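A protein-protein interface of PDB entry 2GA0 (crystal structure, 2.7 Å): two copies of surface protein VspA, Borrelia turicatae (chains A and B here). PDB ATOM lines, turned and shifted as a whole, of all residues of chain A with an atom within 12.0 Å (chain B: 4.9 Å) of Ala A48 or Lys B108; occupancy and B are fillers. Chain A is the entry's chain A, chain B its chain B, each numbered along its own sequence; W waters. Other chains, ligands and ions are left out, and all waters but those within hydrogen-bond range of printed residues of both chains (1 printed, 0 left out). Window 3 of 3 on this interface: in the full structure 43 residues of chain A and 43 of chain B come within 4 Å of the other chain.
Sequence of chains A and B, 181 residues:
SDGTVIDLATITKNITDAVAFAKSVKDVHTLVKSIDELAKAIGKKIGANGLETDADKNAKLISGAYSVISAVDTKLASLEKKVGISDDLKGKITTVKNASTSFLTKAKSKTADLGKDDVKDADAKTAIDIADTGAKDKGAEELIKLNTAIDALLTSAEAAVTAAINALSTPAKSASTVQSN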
ATOM      1  N   LYS A  44      32.948  22.324 -36.952  1.00  0.00           N
ATOM      2  CA  LYS A  44      32.363  23.114 -35.867  1.00  0.00           C
ATOM      3  C   LYS A  44      32.771  22.563 -34.502  1.00  0.00           C
ATOM      4  O   LYS A  44      32.864  21.352 -34.311  1.00  0.00           O
ATOM      5  CB  LYS A  44      30.835  23.148 -35.959  1.00  0.00           C
ATOM      6  CG  LYS A  44      30.274  23.609 -37.282  1.00  0.00           C
ATOM      7  CD  LYS A  44      29.975  25.085 -37.250  1.00  0.00           C
ATOM      8  CE  LYS A  44      29.776  25.654 -38.645  1.00  0.00           C
ATOM      9  NZ  LYS A  44      28.543  25.029 -39.215  1.00  0.00           N
ATOM     10  N   LYS A  45      33.033  23.466 -33.566  1.00  0.00           N
ATOM     11  CA  LYS A  45      33.236  23.089 -32.179  1.00  0.00           C
ATOM     12  C   LYS A  45      32.047  23.498 -31.350  1.00  0.00           C
ATOM     13  O   LYS A  45      31.318  24.382 -31.733  1.00  0.00           O
ATOM     14  CB  LYS A  45      34.504  23.713 -31.598  1.00  0.00           C
ATOM     15  CG  LYS A  45      34.375  25.149 -31.128  1.00  0.00           C
ATOM     16  CD  LYS A  45      35.752  25.768 -30.947  1.00  0.00           C
ATOM     17  CE  LYS A  45      35.743  26.999 -30.040  1.00  0.00           C
ATOM     18  NZ  LYS A  45      36.901  26.949 -29.096  1.00  0.00           N
ATOM     19  N   ILE A  46      31.833  22.846 -30.221  1.00  0.00           N
ATOM     20  CA  ILE A  46      30.863  23.347 -29.275  1.00  0.00           C
ATOM     21  C   ILE A  46      31.495  24.501 -28.539  1.00  0.00           C
ATOM     22  O   ILE A  46      32.618  24.401 -27.991  1.00  0.00           O
ATOM     23  CB  ILE A  46      30.352  22.277 -28.323  1.00  0.00           C
ATOM     24  CG1 ILE A  46      29.735  21.135 -29.107  1.00  0.00           C
ATOM     25  CG2 ILE A  46      29.371  22.900 -27.340  1.00  0.00           C
ATOM     26  CD1 ILE A  46      29.952  19.791 -28.519  1.00  0.00           C
ATOM     27  N   GLY A  47      30.789  25.621 -28.586  1.00  0.00           N
ATOM     28  CA  GLY A  47      31.243  26.872 -28.013  1.00  0.00           C
ATOM     29  C   GLY A  47      30.251  27.348 -26.972  1.00  0.00           C
ATOM     30  O   GLY A  47      29.167  26.769 -26.819  1.00  0.00           O
ATOM     31  N   ALA A  48      30.606  28.408 -26.261  1.00  0.00           N
ATOM     32  CA  ALA A  48      29.775  28.866 -25.166  1.00  0.00           C
ATOM     33  C   ALA A  48      28.315  29.089 -25.572  1.00  0.00           C
ATOM     34  O   ALA A  48      27.453  29.094 -24.707  1.00  0.00           O
ATOM     35  CB  ALA A  48      30.353  30.114 -24.561  1.00  0.00           C
ATOM     36  N   ASN A  49      28.048  29.281 -26.867  1.00  0.00           N
ATOM     37  CA  ASN A  49      26.697  29.618 -27.352  1.00  0.00           C
ATOM     38  C   ASN A  49      26.133  28.647 -28.407  1.00  0.00           C
ATOM     39  O   ASN A  49      25.122  28.928 -29.066  1.00  0.00           O
ATOM     40  CB  ASN A  49      26.684  31.009 -27.960  1.00  0.00           C
ATOM     41  CG  ASN A  49      26.672  32.102 -26.921  1.00  0.00           C
ATOM     42  OD1 ASN A  49      25.783  32.152 -26.067  1.00  0.00           O
ATOM     43  ND2 ASN A  49      27.651  33.011 -27.000  1.00  0.00           N
ATOM     44  N   GLY A  50      26.786  27.509 -28.572  1.00  0.00           N
ATOM     45  CA  GLY A  50      26.344  26.602 -29.588  1.00  0.00           C
ATOM     46  C   GLY A  50      27.490  26.316 -30.508  1.00  0.00           C
ATOM     47  O   GLY A  50      28.634  26.669 -30.206  1.00  0.00           O
ATOM     48  N   LEU A  51      27.201  25.654 -31.617  1.00  0.00           N
ATOM     49  CA  LEU A  51      28.272  25.314 -32.533  1.00  0.00           C
ATOM     50  C   LEU A  51      28.832  26.600 -33.091  1.00  0.00           C
ATOM     51  O   LEU A  51      28.124  27.567 -33.331  1.00  0.00           O
ATOM     52  CB  LEU A  51      27.805  24.383 -33.651  1.00  0.00           C
ATOM     53  CG  LEU A  51      27.220  23.037 -33.198  1.00  0.00           C
ATOM     54  CD1 LEU A  51      26.689  22.296 -34.402  1.00  0.00           C
ATOM     55  CD2 LEU A  51      28.233  22.219 -32.443  1.00  0.00           C
ATOM     56  N   GLU A  52      30.139  26.630 -33.215  1.00  0.00           N
ATOM     57  CA  GLU A  52      30.804  27.714 -33.939  1.00  0.00           C
ATOM     58  C   GLU A  52      31.940  27.124 -34.762  1.00  0.00           C
ATOM     59  O   GLU A  52      32.316  25.943 -34.597  1.00  0.00           O
ATOM     60  CB  GLU A  52      31.268  28.832 -33.033  1.00  0.00           C
ATOM     61  CG  GLU A  52      31.952  28.376 -31.781  1.00  0.00           C
ATOM     62  CD  GLU A  52      32.560  29.550 -31.067  1.00  0.00           C
ATOM     63  OE1 GLU A  52      33.784  29.770 -31.244  1.00  0.00           O
ATOM     64  OE2 GLU A  52      31.804  30.270 -30.381  1.00  0.00           O
ATOM     65  N   THR A  53      32.435  27.922 -35.696  1.00  0.00           N
ATOM     66  CA  THR A  53      33.417  27.449 -36.672  1.00  0.00           C
ATOM     67  C   THR A  53      34.738  27.090 -36.021  1.00  0.00           C
ATOM     68  O   THR A  53      35.281  27.861 -35.203  1.00  0.00           O
ATOM     69  CB  THR A  53      33.671  28.501 -37.761  1.00  0.00           C
ATOM     70  OG1 THR A  53      32.471  28.694 -38.509  1.00  0.00           O
ATOM     71  CG2 THR A  53      34.633  27.972 -38.810  1.00  0.00           C
ATOM     72  N   ASP A  54      35.240  25.925 -36.385  1.00  0.00           N
ATOM     73  CA  ASP A  54      36.561  25.509 -36.022  1.00  0.00           C
ATOM     74  C   ASP A  54      36.933  24.426 -37.030  1.00  0.00           C
ATOM     75  O   ASP A  54      36.744  23.223 -36.812  1.00  0.00           O
ATOM     76  CB  ASP A  54      36.599  25.048 -34.556  1.00  0.00           C
ATOM     77  CG  ASP A  54      37.962  24.489 -34.131  1.00  0.00           C
ATOM     78  OD1 ASP A  54      37.975  23.480 -33.434  1.00  0.00           O
ATOM     79  OD2 ASP A  54      39.067  24.987 -34.409  1.00  0.00           O
ATOM     80  N   TYR B  66      25.990  17.026 -30.361  1.00  0.00           N
ATOM     81  CA  TYR B  66      25.337  18.268 -29.981  1.00  0.00           C
ATOM     82  C   TYR B  66      24.333  18.642 -31.092  1.00  0.00           C
ATOM     83  O   TYR B  66      23.185  19.017 -30.810  1.00  0.00           O
ATOM     84  CB  TYR B  66      26.394  19.362 -29.662  1.00  0.00           C
ATOM     85  CG  TYR B  66      25.849  20.684 -29.232  1.00  0.00           C
ATOM     86  CD1 TYR B  66      25.768  21.027 -27.890  1.00  0.00           C
ATOM     87  CD2 TYR B  66      25.412  21.610 -30.176  1.00  0.00           C
ATOM     88  CE1 TYR B  66      25.274  22.289 -27.489  1.00  0.00           C
ATOM     89  CE2 TYR B  66      24.866  22.865 -29.798  1.00  0.00           C
ATOM     90  CZ  TYR B  66      24.801  23.185 -28.467  1.00  0.00           C
ATOM     91  OH  TYR B  66      24.293  24.409 -28.132  1.00  0.00           O
ATOM     92  N   LEU B 104      22.175  20.530 -23.809  1.00  0.00           N
ATOM     93  CA  LEU B 104      22.766  21.578 -24.646  1.00  0.00           C
ATOM     94  C   LEU B 104      23.435  22.670 -23.812  1.00  0.00           C
ATOM     95  O   LEU B 104      24.534  23.111 -24.139  1.00  0.00           O
ATOM     96  CB  LEU B 104      21.723  22.188 -25.617  1.00  0.00           C
ATOM     97  CG  LEU B 104      21.079  21.271 -26.675  1.00  0.00           C
ATOM     98  CD1 LEU B 104      19.796  21.909 -27.279  1.00  0.00           C
ATOM     99  CD2 LEU B 104      22.044  20.832 -27.775  1.00  0.00           C
ATOM    100  N   THR B 105      22.766  23.106 -22.739  1.00  0.00           N
ATOM    101  CA  THR B 105      23.311  24.082 -21.829  1.00  0.00           C
ATOM    102  C   THR B 105      24.589  23.575 -21.179  1.00  0.00           C
ATOM    103  O   THR B 105      25.558  24.315 -21.085  1.00  0.00           O
ATOM    104  CB  THR B 105      22.285  24.398 -20.757  1.00  0.00           C
ATOM    105  OG1 THR B 105      21.110  24.930 -21.386  1.00  0.00           O
ATOM    106  CG2 THR B 105      22.786  25.535 -19.801  1.00  0.00           C
ATOM    107  N   LYS B 106      24.595  22.322 -20.730  1.00  0.00           N
ATOM    108  CA  LYS B 106      25.779  21.738 -20.099  1.00  0.00           C
ATOM    109  C   LYS B 106      26.976  21.678 -21.046  1.00  0.00           C
ATOM    110  O   LYS B 106      28.093  22.110 -20.668  1.00  0.00           O
ATOM    111  CB  LYS B 106      25.463  20.354 -19.499  1.00  0.00           C
ATOM    112  CG  LYS B 106      26.628  19.648 -18.795  1.00  0.00           C
ATOM    113  CD  LYS B 106      27.148  20.434 -17.593  1.00  0.00           C
ATOM    114  CE  LYS B 106      26.724  19.805 -16.278  1.00  0.00           C
ATOM    115  NZ  LYS B 106      27.601  20.183 -15.132  1.00  0.00           N
ATOM    116  N   ALA B 107      26.737  21.159 -22.255  1.00  0.00           N
ATOM    117  CA  ALA B 107      27.748  21.047 -23.284  1.00  0.00           C
ATOM    118  C   ALA B 107      28.344  22.417 -23.588  1.00  0.00           C
ATOM    119  O   ALA B 107      29.569  22.596 -23.549  1.00  0.00           O
ATOM    120  CB  ALA B 107      27.174  20.466 -24.514  1.00  0.00           C
ATOM    121  N   LYS B 108      27.481  23.393 -23.856  1.00  0.00           N
ATOM    122  CA  LYS B 108      27.937  24.736 -24.141  1.00  0.00           C
ATOM    123  C   LYS B 108      28.825  25.202 -23.038  1.00  0.00           C
ATOM    124  O   LYS B 108      29.844  25.839 -23.282  1.00  0.00           O
ATOM    125  CB  LYS B 108      26.776  25.706 -24.266  1.00  0.00           C
ATOM    126  CG  LYS B 108      26.186  25.807 -25.658  1.00  0.00           C
ATOM    127  CD  LYS B 108      24.994  26.744 -25.665  1.00  0.00           C
ATOM    128  CE  LYS B 108      23.706  25.994 -25.473  1.00  0.00           C
ATOM    129  NZ  LYS B 108      22.559  26.899 -25.650  1.00  0.00           N
ATOM    130  N   SER B 109      28.447  24.897 -21.807  1.00  0.00           N
ATOM    131  CA  SER B 109      29.170  25.464 -20.670  1.00  0.00           C
ATOM    132  C   SER B 109      30.529  24.781 -20.540  1.00  0.00           C
ATOM    133  O   SER B 109      31.445  25.342 -19.900  1.00  0.00           O
ATOM    134  CB  SER B 109      28.369  25.377 -19.376  1.00  0.00           C
ATOM    135  OG  SER B 109      28.597  24.133 -18.747  1.00  0.00           O
ATOM    136  N   LYS B 110      30.671  23.593 -21.157  1.00  0.00           N
ATOM    137  CA  LYS B 110      31.972  22.891 -21.168  1.00  0.00           C
ATOM    138  C   LYS B 110      32.739  23.057 -22.495  1.00  0.00           C
ATOM    139  O   LYS B 110      33.559  22.198 -22.872  1.00  0.00           O
ATOM    140  CB  LYS B 110      31.834  21.407 -20.804  1.00  0.00           C
ATOM    141  CG  LYS B 110      31.152  21.122 -19.476  1.00  0.00           C
ATOM    142  CD  LYS B 110      31.997  21.647 -18.362  1.00  0.00           C
ATOM    143  CE  LYS B 110      31.444  21.308 -16.976  1.00  0.00           C
ATOM    144  NZ  LYS B 110      32.515  21.455 -15.961  1.00  0.00           N
ATOM    145  N   THR B 111      32.488  24.177 -23.183  1.00  0.00           N
ATOM    146  CA  THR B 111      33.182  24.502 -24.423  1.00  0.00           C
ATOM    147  C   THR B 111      34.700  24.337 -24.311  1.00  0.00           C
ATOM    148  O   THR B 111      35.317  23.704 -25.164  1.00  0.00           O
ATOM    149  CB  THR B 111      32.834  25.931 -24.908  1.00  0.00           C
ATOM    150  OG1 THR B 111      33.526  26.193 -26.136  1.00  0.00           O
ATOM    151  CG2 THR B 111      33.349  26.988 -23.963  1.00  0.00           C
HETATM  152  O   HOH W   1      36.805  25.405 -27.161  1.00  0.00           O
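O of Ile A46 sits at hydrogen-bond distance from OG1 of Thr B111, at 2.7 Å.
Among the printed residues, merely in contact across the chains: Gly A47 with Thr B111, Gly A50 with Tyr B66, Gly A47 with Lys B108, Gly A50 with Lys B108, Ala A48 with Lys B108, Asn A49 with Lys B108, Ala A48 with Thr B111, Leu A51 with Tyr B66, Ile A46 with Tyr B66, Ile A46 with Ala B107 and Ile A46 with Lys B108.
Ala A48 touches two residues of chain B.
Lys B108 touches five residues of chain A.
No residue of chain A comes within 4 Å of Leu B104.
No residue of chain A comes within 4 Å of Thr B105.
No residue of chain A comes within 4 Å of Ser B109.
Of the printed residues of chain B, Gly A47 touches Lys B108 (3.3 Å) and Thr B111 (3.0 Å).
Of the printed residues of chain B, Leu A51 touches Tyr B66 (3.7 Å).
The nearest printed residue of chain B that does not touch Leu A51 is Lys B108 (6.0 Å).
Of the 9 printed residues of chain B, 4 touch a printed residue of chain A.
Hydrophobic or aromatic side chains of chain B within 4 Å of the printed part of chain A: Tyr B66.
Along chain B the printed residues that touch a printed residue of chain A span positions 66 to 111.
Hydrophobic or aromatic side chains of chain A that line the printed part of chain B: Ile A46 and Leu A51.
Among the printed residues, 12 pairs touch across the chains.
Among the printed residues, no Asp or Glu carboxylate lies within 4 Å of a Lys or Arg side-chain nitrogen of the other chain.
No position is printed for both chains.
Of the 12 pairs that touch across the chains among the printed residues, none has its exchanged pair printed and touching as well.
Water W1 bridges the side-chain amino group of Lys A45 (2.5 Å) and the backbone carbonyl oxygen of Thr B111 (3.0 Å).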
